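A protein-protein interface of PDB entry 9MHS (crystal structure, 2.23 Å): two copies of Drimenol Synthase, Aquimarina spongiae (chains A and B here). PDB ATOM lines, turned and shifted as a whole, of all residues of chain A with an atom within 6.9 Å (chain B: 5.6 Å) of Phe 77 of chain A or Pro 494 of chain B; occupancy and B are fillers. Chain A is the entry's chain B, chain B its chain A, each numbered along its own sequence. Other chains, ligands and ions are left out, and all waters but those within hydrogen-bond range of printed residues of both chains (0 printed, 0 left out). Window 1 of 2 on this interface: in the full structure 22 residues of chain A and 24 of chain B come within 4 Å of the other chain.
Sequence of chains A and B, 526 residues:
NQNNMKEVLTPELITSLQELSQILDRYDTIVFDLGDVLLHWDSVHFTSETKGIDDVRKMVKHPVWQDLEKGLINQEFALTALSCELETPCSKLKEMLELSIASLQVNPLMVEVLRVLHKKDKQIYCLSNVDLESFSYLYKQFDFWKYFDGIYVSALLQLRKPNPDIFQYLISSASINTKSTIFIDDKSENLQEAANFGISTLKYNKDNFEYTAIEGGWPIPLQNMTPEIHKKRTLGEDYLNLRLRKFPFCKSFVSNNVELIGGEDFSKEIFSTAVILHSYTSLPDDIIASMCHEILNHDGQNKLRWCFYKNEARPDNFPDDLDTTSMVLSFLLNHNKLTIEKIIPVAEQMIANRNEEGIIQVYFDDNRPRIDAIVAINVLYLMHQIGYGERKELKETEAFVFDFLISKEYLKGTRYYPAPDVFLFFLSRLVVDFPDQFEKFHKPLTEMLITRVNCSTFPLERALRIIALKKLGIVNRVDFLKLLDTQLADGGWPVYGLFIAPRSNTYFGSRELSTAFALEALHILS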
ATOM      1  N   VAL A  64     -17.344 -23.057  10.900  1.00  0.00           N
ATOM      2  CA  VAL A  64     -16.454 -22.048  11.471  1.00  0.00           C
ATOM      3  C   VAL A  64     -17.059 -21.479  12.753  1.00  0.00           C
ATOM      4  O   VAL A  64     -16.345 -21.240  13.737  1.00  0.00           O
ATOM      5  CB  VAL A  64     -16.149 -20.946  10.436  1.00  0.00           C
ATOM      6  CG1 VAL A  64     -15.602 -19.703  11.111  1.00  0.00           C
ATOM      7  CG2 VAL A  64     -15.153 -21.453   9.399  1.00  0.00           C
ATOM      8  N   LEU A  68     -15.584 -20.503  16.733  1.00  0.00           N
ATOM      9  CA  LEU A  68     -15.812 -19.321  17.557  1.00  0.00           C
ATOM     10  C   LEU A  68     -16.498 -19.690  18.868  1.00  0.00           C
ATOM     11  O   LEU A  68     -16.097 -19.229  19.939  1.00  0.00           O
ATOM     12  CB  LEU A  68     -16.642 -18.305  16.781  1.00  0.00           C
ATOM     13  CG  LEU A  68     -17.073 -17.090  17.593  1.00  0.00           C
ATOM     14  CD1 LEU A  68     -15.894 -16.182  17.848  1.00  0.00           C
ATOM     15  CD2 LEU A  68     -18.228 -16.331  16.907  1.00  0.00           C
ATOM     16  N   LEU A  72     -11.890 -20.774  19.973  1.00  0.00           N
ATOM     17  CA  LEU A  72     -10.656 -20.930  19.205  1.00  0.00           C
ATOM     18  C   LEU A  72     -10.317 -19.705  18.368  1.00  0.00           C
ATOM     19  O   LEU A  72      -9.162 -19.546  17.971  1.00  0.00           O
ATOM     20  CB  LEU A  72     -10.744 -22.145  18.284  1.00  0.00           C
ATOM     21  CG  LEU A  72     -11.168 -23.382  19.052  1.00  0.00           C
ATOM     22  CD1 LEU A  72     -11.264 -24.622  18.148  1.00  0.00           C
ATOM     23  CD2 LEU A  72     -10.192 -23.580  20.202  1.00  0.00           C
ATOM     24  N   ILE A  73     -11.294 -18.849  18.086  1.00  0.00           N
ATOM     25  CA  ILE A  73     -11.108 -17.640  17.299  1.00  0.00           C
ATOM     26  C   ILE A  73     -12.047 -16.594  17.878  1.00  0.00           C
ATOM     27  O   ILE A  73     -12.980 -16.921  18.615  1.00  0.00           O
ATOM     28  CB  ILE A  73     -11.413 -17.865  15.799  1.00  0.00           C
ATOM     29  CG1 ILE A  73     -12.849 -18.370  15.624  1.00  0.00           C
ATOM     30  CG2 ILE A  73     -10.437 -18.861  15.169  1.00  0.00           C
ATOM     31  CD1 ILE A  73     -13.229 -18.616  14.182  1.00  0.00           C
ATOM     32  N   ASN A  74     -11.806 -15.327  17.537  1.00  0.00           N
ATOM     33  CA  ASN A  74     -12.686 -14.251  17.971  1.00  0.00           C
ATOM     34  C   ASN A  74     -13.670 -13.893  16.853  1.00  0.00           C
ATOM     35  O   ASN A  74     -13.639 -14.467  15.761  1.00  0.00           O
ATOM     36  CB  ASN A  74     -11.879 -13.032  18.429  1.00  0.00           C
ATOM     37  CG  ASN A  74     -11.201 -12.317  17.285  1.00  0.00           C
ATOM     38  OD1 ASN A  74     -10.697 -12.947  16.357  1.00  0.00           O
ATOM     39  ND2 ASN A  74     -11.190 -10.990  17.341  1.00  0.00           N
ATOM     40  N   GLN A  75     -14.570 -12.939  17.136  1.00  0.00           N
ATOM     41  CA  GLN A  75     -15.655 -12.659  16.199  1.00  0.00           C
ATOM     42  C   GLN A  75     -15.127 -12.136  14.867  1.00  0.00           C
ATOM     43  O   GLN A  75     -15.556 -12.592  13.803  1.00  0.00           O
ATOM     44  CB  GLN A  75     -16.655 -11.671  16.798  1.00  0.00           C
ATOM     45  CG  GLN A  75     -18.014 -12.279  17.097  1.00  0.00           C
ATOM     46  CD  GLN A  75     -18.934 -11.342  17.856  1.00  0.00           C
ATOM     47  OE1 GLN A  75     -19.015 -10.152  17.547  1.00  0.00           O
ATOM     48  NE2 GLN A  75     -19.640 -11.877  18.856  1.00  0.00           N
ATOM     49  N   GLU A  76     -14.208 -11.158  14.909  1.00  0.00           N
ATOM     50  CA  GLU A  76     -13.628 -10.617  13.680  1.00  0.00           C
ATOM     51  C   GLU A  76     -13.080 -11.727  12.801  1.00  0.00           C
ATOM     52  O   GLU A  76     -13.316 -11.753  11.590  1.00  0.00           O
ATOM     53  CB  GLU A  76     -12.514  -9.624  14.009  1.00  0.00           C
ATOM     54  CG  GLU A  76     -12.997  -8.226  14.274  1.00  0.00           C
ATOM     55  CD  GLU A  76     -11.853  -7.242  14.434  1.00  0.00           C
ATOM     56  OE1 GLU A  76     -10.733  -7.683  14.770  1.00  0.00           O
ATOM     57  OE2 GLU A  76     -12.075  -6.032  14.200  1.00  0.00           O
ATOM     58  N   PHE A  77     -12.360 -12.660  13.408  1.00  0.00           N
ATOM     59  CA  PHE A  77     -11.777 -13.774  12.681  1.00  0.00           C
ATOM     60  C   PHE A  77     -12.850 -14.663  12.071  1.00  0.00           C
ATOM     61  O   PHE A  77     -12.713 -15.115  10.929  1.00  0.00           O
ATOM     62  CB  PHE A  77     -10.900 -14.572  13.634  1.00  0.00           C
ATOM     63  CG  PHE A  77      -9.634 -15.035  13.034  1.00  0.00           C
ATOM     64  CD1 PHE A  77      -8.592 -14.148  12.835  1.00  0.00           C
ATOM     65  CD2 PHE A  77      -9.473 -16.365  12.673  1.00  0.00           C
ATOM     66  CE1 PHE A  77      -7.409 -14.573  12.276  1.00  0.00           C
ATOM     67  CE2 PHE A  77      -8.288 -16.799  12.117  1.00  0.00           C
ATOM     68  CZ  PHE A  77      -7.257 -15.905  11.918  1.00  0.00           C
ATOM     69  N   ALA A  78     -13.913 -14.948  12.834  1.00  0.00           N
ATOM     70  CA  ALA A  78     -14.953 -15.857  12.360  1.00  0.00           C
ATOM     71  C   ALA A  78     -15.785 -15.208  11.264  1.00  0.00           C
ATOM     72  O   ALA A  78     -16.132 -15.857  10.272  1.00  0.00           O
ATOM     73  CB  ALA A  78     -15.846 -16.293  13.522  1.00  0.00           C
ATOM     74  N   LEU A  79     -16.115 -13.929  11.434  1.00  0.00           N
ATOM     75  CA  LEU A  79     -16.849 -13.197  10.412  1.00  0.00           C
ATOM     76  C   LEU A  79     -16.055 -13.123   9.116  1.00  0.00           C
ATOM     77  O   LEU A  79     -16.597 -13.370   8.034  1.00  0.00           O
ATOM     78  CB  LEU A  79     -17.179 -11.791  10.914  1.00  0.00           C
ATOM     79  CG  LEU A  79     -18.215 -11.751  12.042  1.00  0.00           C
ATOM     80  CD1 LEU A  79     -18.727 -10.349  12.240  1.00  0.00           C
ATOM     81  CD2 LEU A  79     -19.359 -12.691  11.730  1.00  0.00           C
ATOM     82  N   THR A  80     -14.769 -12.770   9.209  1.00  0.00           N
ATOM     83  CA  THR A  80     -13.930 -12.677   8.019  1.00  0.00           C
ATOM     84  C   THR A  80     -13.952 -13.984   7.232  1.00  0.00           C
ATOM     85  O   THR A  80     -14.146 -13.988   6.011  1.00  0.00           O
ATOM     86  CB  THR A  80     -12.501 -12.298   8.425  1.00  0.00           C
ATOM     87  OG1 THR A  80     -12.503 -10.972   8.969  1.00  0.00           O
ATOM     88  CG2 THR A  80     -11.561 -12.341   7.232  1.00  0.00           C
ATOM     89  N   ALA A  81     -13.789 -15.111   7.927  1.00  0.00           N
ATOM     90  CA  ALA A  81     -13.869 -16.397   7.249  1.00  0.00           C
ATOM     91  C   ALA A  81     -15.275 -16.659   6.719  1.00  0.00           C
ATOM     92  O   ALA A  81     -15.434 -17.141   5.590  1.00  0.00           O
ATOM     93  CB  ALA A  81     -13.434 -17.511   8.192  1.00  0.00           C
ATOM     94  N   LEU A  82     -16.308 -16.359   7.521  1.00  0.00           N
ATOM     95  CA  LEU A  82     -17.683 -16.611   7.092  1.00  0.00           C
ATOM     96  C   LEU A  82     -18.060 -15.738   5.909  1.00  0.00           C
ATOM     97  O   LEU A  82     -18.901 -16.128   5.088  1.00  0.00           O
ATOM     98  CB  LEU A  82     -18.665 -16.373   8.240  1.00  0.00           C
ATOM     99  CG  LEU A  82     -18.784 -17.503   9.263  1.00  0.00           C
ATOM    100  CD1 LEU A  82     -19.699 -17.095  10.414  1.00  0.00           C
ATOM    101  CD2 LEU A  82     -19.288 -18.775   8.625  1.00  0.00           C
ATOM    102  N   GLU A 133     -17.419 -12.946  23.043  1.00  0.00           N
ATOM    103  CA  GLU A 133     -17.941 -11.590  22.889  1.00  0.00           C
ATOM    104  C   GLU A 133     -19.431 -11.531  23.184  1.00  0.00           C
ATOM    105  O   GLU A 133     -19.902 -10.625  23.883  1.00  0.00           O
ATOM    106  CB  GLU A 133     -17.673 -11.052  21.487  1.00  0.00           C
ATOM    107  CG  GLU A 133     -16.238 -10.693  21.267  1.00  0.00           C
ATOM    108  CD  GLU A 133     -15.499 -11.704  20.408  1.00  0.00           C
ATOM    109  OE1 GLU A 133     -15.782 -12.937  20.515  1.00  0.00           O
ATOM    110  OE2 GLU A 133     -14.643 -11.253  19.624  1.00  0.00           O
ATOM    111  N   GLU B 259      -4.228  -9.681   8.231  1.00  0.00           N
ATOM    112  CA  GLU B 259      -5.235 -10.698   8.472  1.00  0.00           C
ATOM    113  C   GLU B 259      -6.479 -10.468   7.647  1.00  0.00           C
ATOM    114  O   GLU B 259      -7.411 -11.277   7.721  1.00  0.00           O
ATOM    115  CB  GLU B 259      -5.596 -10.748   9.950  1.00  0.00           C
ATOM    116  CG  GLU B 259      -4.594 -11.508  10.760  1.00  0.00           C
ATOM    117  CD  GLU B 259      -4.470 -10.961  12.153  1.00  0.00           C
ATOM    118  OE1 GLU B 259      -4.268  -9.732  12.289  1.00  0.00           O
ATOM    119  OE2 GLU B 259      -4.598 -11.757  13.102  1.00  0.00           O
ATOM    120  N   ILE B 261      -8.896  -8.619   8.010  1.00  0.00           N
ATOM    121  CA  ILE B 261     -10.103  -8.432   8.800  1.00  0.00           C
ATOM    122  C   ILE B 261     -10.958  -7.362   8.141  1.00  0.00           C
ATOM    123  O   ILE B 261     -10.471  -6.268   7.817  1.00  0.00           O
ATOM    124  CB  ILE B 261      -9.740  -8.060  10.243  1.00  0.00           C
ATOM    125  CG1 ILE B 261      -9.047  -9.245  10.917  1.00  0.00           C
ATOM    126  CG2 ILE B 261     -10.967  -7.617  11.011  1.00  0.00           C
ATOM    127  CD1 ILE B 261      -9.832 -10.565  10.801  1.00  0.00           C
ATOM    128  N   PRO B 459      -0.386 -18.923  10.189  1.00  0.00           N
ATOM    129  CA  PRO B 459      -0.282 -20.265   9.586  1.00  0.00           C
ATOM    130  C   PRO B 459       0.471 -20.309   8.266  1.00  0.00           C
ATOM    131  O   PRO B 459       1.302 -21.203   8.054  1.00  0.00           O
ATOM    132  CB  PRO B 459      -1.753 -20.658   9.401  1.00  0.00           C
ATOM    133  CG  PRO B 459      -2.442 -19.933  10.533  1.00  0.00           C
ATOM    134  CD  PRO B 459      -1.756 -18.619  10.634  1.00  0.00           C
ATOM    135  N   THR B 486      -4.179 -24.730  13.706  1.00  0.00           N
ATOM    136  CA  THR B 486      -4.883 -23.537  13.257  1.00  0.00           C
ATOM    137  C   THR B 486      -5.795 -23.798  12.066  1.00  0.00           C
ATOM    138  O   THR B 486      -6.414 -22.859  11.558  1.00  0.00           O
ATOM    139  CB  THR B 486      -3.885 -22.425  12.935  1.00  0.00           C
ATOM    140  OG1 THR B 486      -3.000 -22.872  11.907  1.00  0.00           O
ATOM    141  CG2 THR B 486      -3.066 -22.086  14.195  1.00  0.00           C
ATOM    142  N   LEU B 488      -9.189 -24.439  10.475  1.00  0.00           N
ATOM    143  CA  LEU B 488     -10.561 -24.222  10.901  1.00  0.00           C
ATOM    144  C   LEU B 488     -11.406 -25.471  10.646  1.00  0.00           C
ATOM    145  O   LEU B 488     -10.971 -26.439  10.015  1.00  0.00           O
ATOM    146  CB  LEU B 488     -11.154 -23.007  10.202  1.00  0.00           C
ATOM    147  CG  LEU B 488     -10.381 -21.732  10.535  1.00  0.00           C
ATOM    148  CD1 LEU B 488     -11.045 -20.506   9.968  1.00  0.00           C
ATOM    149  CD2 LEU B 488     -10.248 -21.610  12.047  1.00  0.00           C
ATOM    150  N   GLY B 492     -10.412 -25.406   5.994  1.00  0.00           N
ATOM    151  CA  GLY B 492      -9.580 -24.362   5.428  1.00  0.00           C
ATOM    152  C   GLY B 492      -8.860 -23.593   6.523  1.00  0.00           C
ATOM    153  O   GLY B 492      -9.348 -23.489   7.642  1.00  0.00           O
ATOM    154  N   TRP B 493      -7.679 -23.080   6.198  1.00  0.00           N
ATOM    155  CA  TRP B 493      -6.949 -22.200   7.098  1.00  0.00           C
ATOM    156  C   TRP B 493      -7.431 -20.772   6.900  1.00  0.00           C
ATOM    157  O   TRP B 493      -8.208 -20.496   5.984  1.00  0.00           O
ATOM    158  CB  TRP B 493      -5.442 -22.350   6.859  1.00  0.00           C
ATOM    159  CG  TRP B 493      -4.856 -23.540   7.566  1.00  0.00           C
ATOM    160  CD1 TRP B 493      -4.200 -23.541   8.760  1.00  0.00           C
ATOM    161  CD2 TRP B 493      -4.891 -24.905   7.128  1.00  0.00           C
ATOM    162  NE1 TRP B 493      -3.820 -24.820   9.092  1.00  0.00           N
ATOM    163  CE2 TRP B 493      -4.234 -25.675   8.109  1.00  0.00           C
ATOM    164  CE3 TRP B 493      -5.410 -25.549   6.001  1.00  0.00           C
ATOM    165  CZ2 TRP B 493      -4.074 -27.052   7.994  1.00  0.00           C
ATOM    166  CZ3 TRP B 493      -5.253 -26.920   5.889  1.00  0.00           C
ATOM    167  CH2 TRP B 493      -4.590 -27.659   6.886  1.00  0.00           C
ATOM    168  N   PRO B 494      -7.027 -19.838   7.766  1.00  0.00           N
ATOM    169  CA  PRO B 494      -7.535 -18.465   7.661  1.00  0.00           C
ATOM    170  C   PRO B 494      -6.897 -17.704   6.513  1.00  0.00           C
ATOM    171  O   PRO B 494      -5.779 -17.988   6.088  1.00  0.00           O
ATOM    172  CB  PRO B 494      -7.136 -17.824   9.002  1.00  0.00           C
ATOM    173  CG  PRO B 494      -6.807 -18.967   9.905  1.00  0.00           C
ATOM    174  CD  PRO B 494      -6.271 -20.037   9.019  1.00  0.00           C
ATOM    175  N   VAL B 495      -7.621 -16.684   6.051  1.00  0.00           N
ATOM    176  CA  VAL B 495      -7.078 -15.786   5.046  1.00  0.00           C
ATOM    177  C   VAL B 495      -5.796 -15.119   5.576  1.00  0.00           C
ATOM    178  O   VAL B 495      -5.626 -14.889   6.784  1.00  0.00           O
ATOM    179  CB  VAL B 495      -8.137 -14.746   4.643  1.00  0.00           C
ATOM    180  CG1 VAL B 495      -8.461 -13.840   5.821  1.00  0.00           C
ATOM    181  CG2 VAL B 495      -7.690 -13.930   3.389  1.00  0.00           C
ATOM    182  N   TYR B 496      -4.875 -14.835   4.660  1.00  0.00           N
ATOM    183  CA  TYR B 496      -3.618 -14.182   4.988  1.00  0.00           C
ATOM    184  C   TYR B 496      -3.218 -13.260   3.842  1.00  0.00           C
ATOM    185  O   TYR B 496      -3.360 -13.616   2.670  1.00  0.00           O
ATOM    186  CB  TYR B 496      -2.510 -15.210   5.258  1.00  0.00           C
ATOM    187  CG  TYR B 496      -1.155 -14.582   5.503  1.00  0.00           C
ATOM    188  CD1 TYR B 496      -0.305 -14.261   4.439  1.00  0.00           C
ATOM    189  CD2 TYR B 496      -0.720 -14.305   6.800  1.00  0.00           C
ATOM    190  CE1 TYR B 496       0.927 -13.687   4.664  1.00  0.00           C
ATOM    191  CE2 TYR B 496       0.520 -13.733   7.034  1.00  0.00           C
ATOM    192  CZ  TYR B 496       1.337 -13.425   5.963  1.00  0.00           C
ATOM    193  OH  TYR B 496       2.564 -12.848   6.187  1.00  0.00           O
ATOM    194  N   SER B 510      -6.276 -14.912   0.357  1.00  0.00           N
ATOM    195  CA  SER B 510      -7.442 -15.770   0.245  1.00  0.00           C
ATOM    196  C   SER B 510      -7.247 -16.979   1.138  1.00  0.00           C
ATOM    197  O   SER B 510      -6.117 -17.362   1.456  1.00  0.00           O
ATOM    198  CB  SER B 510      -7.664 -16.210  -1.202  1.00  0.00           C
ATOM    199  OG  SER B 510      -6.602 -17.057  -1.633  1.00  0.00           O
ATOM    200  N   ARG B 511      -8.367 -17.590   1.527  1.00  0.00           N
ATOM    201  CA  ARG B 511      -8.278 -18.869   2.219  1.00  0.00           C
ATOM    202  C   ARG B 511      -7.654 -19.924   1.317  1.00  0.00           C
ATOM    203  O   ARG B 511      -6.915 -20.794   1.790  1.00  0.00           O
ATOM    204  CB  ARG B 511      -9.661 -19.324   2.699  1.00  0.00           C
ATOM    205  CG  ARG B 511     -10.332 -18.368   3.681  1.00  0.00           C
ATOM    206  CD  ARG B 511     -11.523 -19.023   4.363  1.00  0.00           C
ATOM    207  NE  ARG B 511     -11.113 -20.127   5.229  1.00  0.00           N
ATOM    208  CZ  ARG B 511     -11.952 -21.012   5.750  1.00  0.00           C
ATOM    209  NH1 ARG B 511     -13.248 -20.963   5.492  1.00  0.00           N
ATOM    210  NH2 ARG B 511     -11.482 -21.966   6.556  1.00  0.00           N
ATOM    211  N   SER B 514      -3.785 -19.614   1.617  1.00  0.00           N
ATOM    212  CA  SER B 514      -3.352 -20.157   2.896  1.00  0.00           C
ATOM    213  C   SER B 514      -3.450 -21.675   2.916  1.00  0.00           C
ATOM    214  O   SER B 514      -2.486 -22.360   3.263  1.00  0.00           O
ATOM    215  CB  SER B 514      -4.183 -19.550   4.017  1.00  0.00           C
ATOM    216  OG  SER B 514      -3.844 -18.193   4.197  1.00  0.00           O
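The side-chain amide oxygen (OD1) of Asn 74 of chain A sits close to the backbone NH (N) of Phe 77 of chain A (3.4 Å). The backbone carbonyl oxygen (O) of Glu 76 of chain A sits at hydrogen-bond distance from the side-chain hydroxyl (OG1) of Thr 80 of chain A (2.9 Å). The backbone carbonyl oxygen of Pro 494 of chain B is in hydrogen-bond range of the side-chain hydroxyl of Ser 514 of chain B.
Among the printed residues, pairs that only touch across the chains: Thr 80 of chain A with Ile 261 of chain B (3.3 Å), Phe 77 of chain A with Pro 494 of chain B (3.4 Å), Glu 76 of chain A with Ile 261 of chain B (3.6 Å) and Thr 80 of chain A with Val 495 of chain B (3.7 Å).
Phe 77 of chain A touches just one residue of chain B: Pro 494 (3.4 Å). Printed residues of chain B within 4 Å of Thr 80 of chain A: Ile 261 (3.3 Å) and Val 495 (3.7 Å). Printed residues of chain A within 4 Å of Ile 261 of chain B: Glu 76 (3.6 Å) and Thr 80 (3.3 Å). Pro 494 of chain B touches one residue of chain A. Printed residues of chain A within 4 Å of Val 495 of chain B: Thr 80 (3.7 Å). The nearest printed residue of chain A that does not touch Val 495 of chain B is Phe 77 of chain A (5.5 Å).
Hydrophobic or aromatic side chains of chain A that line the printed part of chain B: Phe 77. Of the 13 printed residues of chain B, 3 touch a printed residue of chain A. Printed residues of chain B that touch a printed residue of chain A: Ile 261, Pro 494 and Val 495. Hydrophobic or aromatic side chains of chain B that line the printed part of chain A: Ile 261, Pro 494 and Val 495. Among the printed residues, 4 pairs touch across the chains. Among the printed residues, no Asp or Glu carboxylate lies within 4 Å of a Lys or Arg side-chain nitrogen of the other chain.
No position is printed for both chains.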
